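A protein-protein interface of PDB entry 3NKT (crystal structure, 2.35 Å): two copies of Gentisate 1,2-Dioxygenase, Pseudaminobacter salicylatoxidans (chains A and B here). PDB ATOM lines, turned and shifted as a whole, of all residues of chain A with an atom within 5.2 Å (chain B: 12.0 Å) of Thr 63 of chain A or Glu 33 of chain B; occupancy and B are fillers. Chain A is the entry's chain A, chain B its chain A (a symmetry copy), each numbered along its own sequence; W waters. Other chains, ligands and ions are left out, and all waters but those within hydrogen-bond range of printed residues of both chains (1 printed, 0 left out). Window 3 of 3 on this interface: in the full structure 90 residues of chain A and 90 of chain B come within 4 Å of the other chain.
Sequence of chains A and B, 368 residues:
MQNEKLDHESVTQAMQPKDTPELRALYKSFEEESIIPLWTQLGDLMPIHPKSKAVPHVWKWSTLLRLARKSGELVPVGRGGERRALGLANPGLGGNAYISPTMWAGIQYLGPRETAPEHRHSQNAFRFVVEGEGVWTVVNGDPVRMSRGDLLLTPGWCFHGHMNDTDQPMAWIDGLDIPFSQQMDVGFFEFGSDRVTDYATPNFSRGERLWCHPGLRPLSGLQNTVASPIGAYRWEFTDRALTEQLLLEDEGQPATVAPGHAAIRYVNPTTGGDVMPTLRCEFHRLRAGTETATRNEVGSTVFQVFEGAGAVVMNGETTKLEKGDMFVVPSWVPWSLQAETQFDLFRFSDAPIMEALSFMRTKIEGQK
No position is printed for both chains.
Of the 9 pairs that touch across the chains among the printed residues, none has its exchanged pair printed and touching as well.
OE2 of Glu 33 of chain B touches CG2 of Thr 63 of chain A, at 3.6 Å.
CD2 of Leu 64 of chain A touches CD1 of Ile 35 of chain B, 3.6 Å away.
O of Leu 67 of chain A touches CD1 of Leu 26 of chain B (3.97 Å).
Leu 67 of chain A touches Ser 29 of chain B (CD2 to OG, 3.3 Å).
Leu 67 of chain A touches Phe 30 of chain B (CB to CE1, 3.97 Å).
CD1 of Leu 67 of chain A touches CB of Glu 33 of chain B, at 3.9 Å.
CG1 of Ile 35 of chain B touches CD1 of Leu 67 of chain A, at 3.9 Å.
Water W1 bridges the guanidinium group (NH2) of Arg 66 of chain A (2.6 Å) and the side-chain hydroxyl (OG) of Ser 29 of chain B (3.4 Å).
Of the 10 printed residues of chain A, 4 touch a printed residue of chain B.
Printed residues of chain A that touch a printed residue of chain B: Trp 59, Thr 63, Leu 64 and Leu 67.
Hydrophobic or aromatic side chains of chain B that line the printed part of chain A: Leu 26, Phe 30 and Ile 35.
Among the printed residues, no Asp or Glu carboxylate lies within 4 Å of a Lys or Arg side-chain nitrogen of the other chain.
The indole nitrogen of Trp 59 of chain A is in hydrogen-bond range of the backbone carbonyl oxygen of Glu 33 of chain B (3.1 Å).
NE1 of Trp 59 of chain A lies within hydrogen-bond range of O of Ser 34 of chain B.
Thr 63 of chain A touches just one residue of chain B: Glu 33.
No residue of chain B comes within 4 Å of Leu 65 of chain A.
No residue of chain B comes within 4 Å of Arg 66 of chain A.
Of chain B, only Leu 26 (3.97 Å), Ser 29 (3.3 Å), Phe 30 (3.97 Å), Glu 33 (3.9 Å) and Ile 35 (3.9 Å) come within 4 Å of Leu 67 of chain A.
Ala 25 of chain B touches none of the printed residues of chain A.
Printed residues of chain A within 4 Å of Leu 26 of chain B: Leu 67.
Printed residues of chain A within 4 Å of Ser 29 of chain B: Leu 67.
Of chain A, only Trp 59 (3.1 Å), Thr 63 (3.6 Å) and Leu 67 (3.9 Å) come within 4 Å of Glu 33 of chain B.
Printed residues of chain A within 4 Å of Ile 35 of chain B: Leu 64 and Leu 67.
The nearest residue of chain B that does not touch Thr 63 of chain A is Ile 35 of chain B (6.2 Å).
The nearest residue of chain A that does not touch Glu 33 of chain B is Arg 66 of chain A (4.6 Å).
The nearest printed residue of chain A that does not touch Ile 35 of chain B is Trp 59 of chain A (4.2 Å).
The backbone NH of Ile 35 of chain B is in hydrogen-bond range of the backbone carbonyl oxygen of Phe 30 of chain B (3.0 Å).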
ATOM      1  N   TRP A  59      -5.014  -4.218  25.586  1.00  0.00           N
ATOM      2  CA  TRP A  59      -5.182  -5.633  25.898  1.00  0.00           C
ATOM      3  C   TRP A  59      -4.009  -6.063  26.770  1.00  0.00           C
ATOM      4  O   TRP A  59      -2.858  -5.709  26.475  1.00  0.00           O
ATOM      5  CB  TRP A  59      -5.187  -6.474  24.625  1.00  0.00           C
ATOM      6  CG  TRP A  59      -6.466  -6.490  23.911  1.00  0.00           C
ATOM      7  CD1 TRP A  59      -7.463  -7.399  24.067  1.00  0.00           C
ATOM      8  CD2 TRP A  59      -6.908  -5.564  22.916  1.00  0.00           C
ATOM      9  NE1 TRP A  59      -8.493  -7.109  23.248  1.00  0.00           N
ATOM     10  CE2 TRP A  59      -8.202  -5.969  22.534  1.00  0.00           C
ATOM     11  CE3 TRP A  59      -6.339  -4.433  22.314  1.00  0.00           C
ATOM     12  CZ2 TRP A  59      -8.951  -5.299  21.541  1.00  0.00           C
ATOM     13  CZ3 TRP A  59      -7.082  -3.753  21.311  1.00  0.00           C
ATOM     14  CH2 TRP A  59      -8.370  -4.198  20.935  1.00  0.00           C
ATOM     15  N   LYS A  60      -4.296  -6.802  27.845  1.00  0.00           N
ATOM     16  CA  LYS A  60      -3.259  -7.172  28.830  1.00  0.00           C
ATOM     17  C   LYS A  60      -2.645  -8.476  28.378  1.00  0.00           C
ATOM     18  O   LYS A  60      -3.337  -9.324  27.863  1.00  0.00           O
ATOM     19  CB  LYS A  60      -3.817  -7.382  30.243  1.00  0.00           C
ATOM     20  CG  LYS A  60      -4.569  -6.198  30.846  1.00  0.00           C
ATOM     21  CD  LYS A  60      -3.613  -5.132  31.304  1.00  0.00           C
ATOM     22  CE  LYS A  60      -4.100  -3.740  30.829  1.00  0.00           C
ATOM     23  NZ  LYS A  60      -3.008  -2.679  30.846  1.00  0.00           N
ATOM     24  N   TRP A  61      -1.346  -8.639  28.599  1.00  0.00           N
ATOM     25  CA  TRP A  61      -0.652  -9.788  28.091  1.00  0.00           C
ATOM     26  C   TRP A  61      -1.013 -11.018  28.915  1.00  0.00           C
ATOM     27  O   TRP A  61      -1.193 -12.106  28.355  1.00  0.00           O
ATOM     28  CB  TRP A  61       0.857  -9.529  28.022  1.00  0.00           C
ATOM     29  CG  TRP A  61       1.681 -10.672  27.466  1.00  0.00           C
ATOM     30  CD1 TRP A  61       2.555 -11.459  28.162  1.00  0.00           C
ATOM     31  CD2 TRP A  61       1.711 -11.146  26.109  1.00  0.00           C
ATOM     32  NE1 TRP A  61       3.134 -12.380  27.324  1.00  0.00           N
ATOM     33  CE2 TRP A  61       2.622 -12.221  26.064  1.00  0.00           C
ATOM     34  CE3 TRP A  61       1.037 -10.778  24.930  1.00  0.00           C
ATOM     35  CZ2 TRP A  61       2.900 -12.923  24.880  1.00  0.00           C
ATOM     36  CZ3 TRP A  61       1.310 -11.464  23.753  1.00  0.00           C
ATOM     37  CH2 TRP A  61       2.243 -12.525  23.735  1.00  0.00           C
ATOM     38  N   SER A  62      -1.170 -10.855  30.227  1.00  0.00           N
ATOM     39  CA  SER A  62      -1.577 -11.981  31.069  1.00  0.00           C
ATOM     40  C   SER A  62      -2.933 -12.551  30.581  1.00  0.00           C
ATOM     41  O   SER A  62      -3.104 -13.783  30.514  1.00  0.00           O
ATOM     42  CB  SER A  62      -1.632 -11.583  32.543  1.00  0.00           C
ATOM     43  OG  SER A  62      -2.448 -10.428  32.729  1.00  0.00           O
ATOM     44  N   THR A  63      -3.873 -11.667  30.232  1.00  0.00           N
ATOM     45  CA  THR A  63      -5.144 -12.081  29.648  1.00  0.00           C
ATOM     46  C   THR A  63      -4.916 -12.779  28.293  1.00  0.00           C
ATOM     47  O   THR A  63      -5.525 -13.825  28.022  1.00  0.00           O
ATOM     48  CB  THR A  63      -6.168 -10.899  29.491  1.00  0.00           C
ATOM     49  OG1 THR A  63      -6.489 -10.346  30.772  1.00  0.00           O
ATOM     50  CG2 THR A  63      -7.466 -11.365  28.860  1.00  0.00           C
ATOM     51  N   LEU A  64      -4.052 -12.218  27.443  1.00  0.00           N
ATOM     52  CA  LEU A  64      -3.849 -12.808  26.111  1.00  0.00           C
ATOM     53  C   LEU A  64      -3.186 -14.180  26.234  1.00  0.00           C
ATOM     54  O   LEU A  64      -3.574 -15.109  25.540  1.00  0.00           O
ATOM     55  CB  LEU A  64      -3.103 -11.859  25.145  1.00  0.00           C
ATOM     56  CG  LEU A  64      -3.738 -10.489  24.785  1.00  0.00           C
ATOM     57  CD1 LEU A  64      -2.814  -9.723  23.885  1.00  0.00           C
ATOM     58  CD2 LEU A  64      -5.135 -10.601  24.138  1.00  0.00           C
ATOM     59  N   LEU A  65      -2.228 -14.288  27.152  1.00  0.00           N
ATOM     60  CA  LEU A  65      -1.540 -15.530  27.459  1.00  0.00           C
ATOM     61  C   LEU A  65      -2.448 -16.656  27.981  1.00  0.00           C
ATOM     62  O   LEU A  65      -2.489 -17.767  27.407  1.00  0.00           O
ATOM     63  CB  LEU A  65      -0.410 -15.275  28.448  1.00  0.00           C
ATOM     64  CG  LEU A  65       0.973 -15.264  27.792  1.00  0.00           C
ATOM     65  CD1 LEU A  65       2.040 -15.065  28.848  1.00  0.00           C
ATOM     66  CD2 LEU A  65       1.226 -16.555  27.005  1.00  0.00           C
ATOM     67  N   ARG A  66      -3.191 -16.371  29.039  1.00  0.00           N
ATOM     68  CA  ARG A  66      -4.147 -17.323  29.572  1.00  0.00           C
ATOM     69  C   ARG A  66      -5.085 -17.855  28.458  1.00  0.00           C
ATOM     70  O   ARG A  66      -5.227 -19.084  28.317  1.00  0.00           O
ATOM     71  CB  ARG A  66      -4.929 -16.689  30.729  1.00  0.00           C
ATOM     72  CG  ARG A  66      -5.674 -17.668  31.651  1.00  0.00           C
ATOM     73  CD  ARG A  66      -6.403 -16.959  32.815  1.00  0.00           C
ATOM     74  NE  ARG A  66      -7.474 -16.121  32.286  1.00  0.00           N
ATOM     75  CZ  ARG A  66      -7.443 -14.782  32.265  1.00  0.00           C
ATOM     76  NH1 ARG A  66      -6.396 -14.129  32.802  1.00  0.00           N
ATOM     77  NH2 ARG A  66      -8.461 -14.098  31.707  1.00  0.00           N
ATOM     78  N   LEU A  67      -5.684 -16.963  27.651  1.00  0.00           N
ATOM     79  CA  LEU A  67      -6.623 -17.389  26.588  1.00  0.00           C
ATOM     80  C   LEU A  67      -5.950 -18.170  25.434  1.00  0.00           C
ATOM     81  O   LEU A  67      -6.530 -19.112  24.892  1.00  0.00           O
ATOM     82  CB  LEU A  67      -7.405 -16.208  26.001  1.00  0.00           C
ATOM     83  CG  LEU A  67      -8.276 -15.246  26.833  1.00  0.00           C
ATOM     84  CD1 LEU A  67      -8.848 -14.129  25.959  1.00  0.00           C
ATOM     85  CD2 LEU A  67      -9.393 -15.968  27.569  1.00  0.00           C
ATOM     86  N   ALA A  68      -4.751 -17.768  25.041  1.00  0.00           N
ATOM     87  CA  ALA A  68      -4.016 -18.499  24.026  1.00  0.00           C
ATOM     88  C   ALA A  68      -3.610 -19.891  24.538  1.00  0.00           C
ATOM     89  O   ALA A  68      -3.715 -20.867  23.806  1.00  0.00           O
ATOM     90  CB  ALA A  68      -2.811 -17.707  23.540  1.00  0.00           C
ATOM     91  N   ARG B  24     -17.048 -23.839  25.255  1.00  0.00           N
ATOM     92  CA  ARG B  24     -18.078 -22.791  25.224  1.00  0.00           C
ATOM     93  C   ARG B  24     -17.723 -21.650  26.189  1.00  0.00           C
ATOM     94  O   ARG B  24     -17.924 -20.491  25.852  1.00  0.00           O
ATOM     95  CB  ARG B  24     -19.473 -23.373  25.524  1.00  0.00           C
ATOM     96  CG  ARG B  24     -20.369 -23.556  24.321  1.00  0.00           C
ATOM     97  CD  ARG B  24     -21.671 -24.281  24.710  1.00  0.00           C
ATOM     98  NE  ARG B  24     -21.456 -25.686  24.432  1.00  0.00           N
ATOM     99  CZ  ARG B  24     -21.532 -26.702  25.288  1.00  0.00           C
ATOM    100  NH1 ARG B  24     -21.879 -26.557  26.551  1.00  0.00           N
ATOM    101  NH2 ARG B  24     -21.246 -27.900  24.830  1.00  0.00           N
ATOM    102  N   ALA B  25     -17.182 -21.995  27.360  1.00  0.00           N
ATOM    103  CA  ALA B  25     -16.662 -21.030  28.310  1.00  0.00           C
ATOM    104  C   ALA B  25     -15.470 -20.221  27.748  1.00  0.00           C
ATOM    105  O   ALA B  25     -15.320 -19.042  28.053  1.00  0.00           O
ATOM    106  CB  ALA B  25     -16.269 -21.721  29.644  1.00  0.00           C
ATOM    107  N   LEU B  26     -14.612 -20.882  26.972  1.00  0.00           N
ATOM    108  CA  LEU B  26     -13.453 -20.234  26.381  1.00  0.00           C
ATOM    109  C   LEU B  26     -13.943 -19.229  25.353  1.00  0.00           C
ATOM    110  O   LEU B  26     -13.382 -18.147  25.274  1.00  0.00           O
ATOM    111  CB  LEU B  26     -12.492 -21.265  25.756  1.00  0.00           C
ATOM    112  CG  LEU B  26     -11.278 -20.793  24.940  1.00  0.00           C
ATOM    113  CD1 LEU B  26     -10.257 -20.103  25.854  1.00  0.00           C
ATOM    114  CD2 LEU B  26     -10.611 -21.916  24.176  1.00  0.00           C
ATOM    115  N   TYR B  27     -14.979 -19.578  24.578  1.00  0.00           N
ATOM    116  CA  TYR B  27     -15.489 -18.685  23.517  1.00  0.00           C
ATOM    117  C   TYR B  27     -16.219 -17.493  24.120  1.00  0.00           C
ATOM    118  O   TYR B  27     -16.106 -16.362  23.628  1.00  0.00           O
ATOM    119  CB  TYR B  27     -16.432 -19.406  22.538  1.00  0.00           C
ATOM    120  CG  TYR B  27     -15.757 -20.269  21.474  1.00  0.00           C
ATOM    121  CD1 TYR B  27     -14.397 -20.543  21.539  1.00  0.00           C
ATOM    122  CD2 TYR B  27     -16.505 -20.860  20.428  1.00  0.00           C
ATOM    123  CE1 TYR B  27     -13.782 -21.337  20.601  1.00  0.00           C
ATOM    124  CE2 TYR B  27     -15.886 -21.678  19.456  1.00  0.00           C
ATOM    125  CZ  TYR B  27     -14.516 -21.907  19.569  1.00  0.00           C
ATOM    126  OH  TYR B  27     -13.831 -22.700  18.675  1.00  0.00           O
ATOM    127  N   LYS B  28     -16.973 -17.756  25.185  1.00  0.00           N
ATOM    128  CA  LYS B  28     -17.591 -16.714  25.982  1.00  0.00           C
ATOM    129  C   LYS B  28     -16.539 -15.771  26.568  1.00  0.00           C
ATOM    130  O   LYS B  28     -16.732 -14.536  26.615  1.00  0.00           O
ATOM    131  CB  LYS B  28     -18.396 -17.356  27.103  1.00  0.00           C
ATOM    132  CG  LYS B  28     -19.009 -16.411  28.124  1.00  0.00           C
ATOM    133  CD  LYS B  28     -20.196 -15.696  27.552  1.00  0.00           C
ATOM    134  CE  LYS B  28     -20.744 -14.698  28.577  1.00  0.00           C
ATOM    135  NZ  LYS B  28     -21.485 -13.560  27.947  1.00  0.00           N
ATOM    136  N   SER B  29     -15.457 -16.356  27.072  1.00  0.00           N
ATOM    137  CA  SER B  29     -14.392 -15.555  27.576  1.00  0.00           C
ATOM    138  C   SER B  29     -13.681 -14.717  26.489  1.00  0.00           C
ATOM    139  O   SER B  29     -13.168 -13.637  26.816  1.00  0.00           O
ATOM    140  CB  SER B  29     -13.396 -16.399  28.316  1.00  0.00           C
ATOM    141  OG  SER B  29     -12.427 -15.523  28.867  1.00  0.00           O
ATOM    142  N   PHE B  30     -13.656 -15.201  25.228  1.00  0.00           N
ATOM    143  CA  PHE B  30     -13.147 -14.427  24.082  1.00  0.00           C
ATOM    144  C   PHE B  30     -13.956 -13.148  23.901  1.00  0.00           C
ATOM    145  O   PHE B  30     -13.366 -12.067  23.848  1.00  0.00           O
ATOM    146  CB  PHE B  30     -13.194 -15.180  22.746  1.00  0.00           C
ATOM    147  CG  PHE B  30     -12.158 -16.262  22.595  1.00  0.00           C
ATOM    148  CD1 PHE B  30     -10.997 -16.267  23.378  1.00  0.00           C
ATOM    149  CD2 PHE B  30     -12.340 -17.277  21.655  1.00  0.00           C
ATOM    150  CE1 PHE B  30     -10.041 -17.286  23.239  1.00  0.00           C
ATOM    151  CE2 PHE B  30     -11.402 -18.271  21.499  1.00  0.00           C
ATOM    152  CZ  PHE B  30     -10.245 -18.281  22.297  1.00  0.00           C
ATOM    153  N   GLU B  31     -15.288 -13.276  23.779  1.00  0.00           N
ATOM    154  CA  GLU B  31     -16.194 -12.130  23.585  1.00  0.00           C
ATOM    155  C   GLU B  31     -15.987 -11.103  24.694  1.00  0.00           C
ATOM    156  O   GLU B  31     -15.982  -9.876  24.429  1.00  0.00           O
ATOM    157  CB  GLU B  31     -17.660 -12.534  23.606  1.00  0.00           C
ATOM    158  CG  GLU B  31     -18.127 -13.472  22.494  1.00  0.00           C
ATOM    159  CD  GLU B  31     -19.354 -14.298  22.932  1.00  0.00           C
ATOM    160  OE1 GLU B  31     -19.435 -15.506  22.591  1.00  0.00           O
ATOM    161  OE2 GLU B  31     -20.213 -13.749  23.659  1.00  0.00           O
ATOM    162  N   GLU B  32     -15.825 -11.589  25.922  1.00  0.00           N
ATOM    163  CA  GLU B  32     -15.619 -10.689  27.046  1.00  0.00           C
ATOM    164  C   GLU B  32     -14.346  -9.854  26.917  1.00  0.00           C
ATOM    165  O   GLU B  32     -14.299  -8.696  27.366  1.00  0.00           O
ATOM    166  CB  GLU B  32     -15.612 -11.437  28.390  1.00  0.00           C
ATOM    167  CG  GLU B  32     -17.008 -11.953  28.812  1.00  0.00           C
ATOM    168  CD  GLU B  32     -16.968 -12.920  30.028  1.00  0.00           C
ATOM    169  OE1 GLU B  32     -18.066 -13.373  30.425  1.00  0.00           O
ATOM    170  OE2 GLU B  32     -15.866 -13.226  30.564  1.00  0.00           O
ATOM    171  N   GLU B  33     -13.321 -10.454  26.309  1.00  0.00           N
ATOM    172  CA  GLU B  33     -12.005  -9.871  26.323  1.00  0.00           C
ATOM    173  C   GLU B  33     -11.646  -9.230  24.986  1.00  0.00           C
ATOM    174  O   GLU B  33     -10.500  -8.885  24.776  1.00  0.00           O
ATOM    175  CB  GLU B  33     -10.950 -10.894  26.735  1.00  0.00           C
ATOM    176  CG  GLU B  33     -11.114 -11.509  28.111  1.00  0.00           C
ATOM    177  CD  GLU B  33     -10.987 -10.541  29.261  1.00  0.00           C
ATOM    178  OE1 GLU B  33     -11.446 -10.909  30.356  1.00  0.00           O
ATOM    179  OE2 GLU B  33     -10.449  -9.420  29.108  1.00  0.00           O
ATOM    180  N   SER B  34     -12.648  -9.070  24.120  1.00  0.00           N
ATOM    181  CA  SER B  34     -12.522  -8.490  22.772  1.00  0.00           C
ATOM    182  C   SER B  34     -11.540  -9.200  21.872  1.00  0.00           C
ATOM    183  O   SER B  34     -10.667  -8.560  21.250  1.00  0.00           O
ATOM    184  CB  SER B  34     -12.203  -7.015  22.849  1.00  0.00           C
ATOM    185  OG  SER B  34     -13.310  -6.411  23.460  1.00  0.00           O
ATOM    186  N   ILE B  35     -11.718 -10.521  21.831  1.00  0.00           N
ATOM    187  CA  ILE B  35     -10.912 -11.482  21.103  1.00  0.00           C
ATOM    188  C   ILE B  35     -11.783 -12.259  20.101  1.00  0.00           C
ATOM    189  O   ILE B  35     -12.882 -12.701  20.455  1.00  0.00           O
ATOM    190  CB  ILE B  35     -10.251 -12.434  22.109  1.00  0.00           C
ATOM    191  CG1 ILE B  35      -9.227 -11.673  22.943  1.00  0.00           C
ATOM    192  CG2 ILE B  35      -9.592 -13.651  21.420  1.00  0.00           C
ATOM    193  CD1 ILE B  35      -8.040 -11.166  22.148  1.00  0.00           C
ATOM    194  N   ILE B  36     -11.331 -12.372  18.847  1.00  0.00           N
ATOM    195  CA  ILE B  36     -12.004 -13.234  17.879  1.00  0.00           C
ATOM    196  C   ILE B  36     -10.982 -14.198  17.267  1.00  0.00           C
ATOM    197  O   ILE B  36     -10.007 -13.775  16.651  1.00  0.00           O
ATOM    198  CB  ILE B  36     -12.752 -12.471  16.788  1.00  0.00           C
ATOM    199  CG1 ILE B  36     -13.815 -11.543  17.398  1.00  0.00           C
ATOM    200  CG2 ILE B  36     -13.447 -13.439  15.845  1.00  0.00           C
ATOM    201  CD1 ILE B  36     -14.425 -10.625  16.382  1.00  0.00           C
ATOM    202  N   PRO B  37     -11.189 -15.504  17.462  1.00  0.00           N
ATOM    203  CA  PRO B  37     -10.246 -16.488  16.959  1.00  0.00           C
ATOM    204  C   PRO B  37     -10.253 -16.536  15.410  1.00  0.00           C
ATOM    205  O   PRO B  37     -11.303 -16.384  14.778  1.00  0.00           O
ATOM    206  CB  PRO B  37     -10.819 -17.796  17.511  1.00  0.00           C
ATOM    207  CG  PRO B  37     -12.307 -17.543  17.573  1.00  0.00           C
ATOM    208  CD  PRO B  37     -12.368 -16.138  18.092  1.00  0.00           C
ATOM    209  N   TRP B  39      -9.734 -19.206  13.584  1.00  0.00           N
ATOM    210  CA  TRP B  39     -10.079 -20.483  12.980  1.00  0.00           C
ATOM    211  C   TRP B  39     -11.568 -20.663  12.619  1.00  0.00           C
ATOM    212  O   TRP B  39     -11.933 -21.556  11.857  1.00  0.00           O
ATOM    213  CB  TRP B  39      -9.551 -21.601  13.857  1.00  0.00           C
ATOM    214  CG  TRP B  39     -10.096 -21.610  15.232  1.00  0.00           C
ATOM    215  CD1 TRP B  39     -11.266 -22.170  15.624  1.00  0.00           C
ATOM    216  CD2 TRP B  39      -9.483 -21.069  16.415  1.00  0.00           C
ATOM    217  NE1 TRP B  39     -11.439 -22.002  16.969  1.00  0.00           N
ATOM    218  CE2 TRP B  39     -10.351 -21.339  17.487  1.00  0.00           C
ATOM    219  CE3 TRP B  39      -8.294 -20.370  16.670  1.00  0.00           C
ATOM    220  CZ2 TRP B  39     -10.067 -20.944  18.821  1.00  0.00           C
ATOM    221  CZ3 TRP B  39      -8.001 -19.976  18.026  1.00  0.00           C
ATOM    222  CH2 TRP B  39      -8.894 -20.263  19.068  1.00  0.00           C
HETATM  223  O   HOH W   1      -9.692 -16.230  30.743  1.00  0.00           O
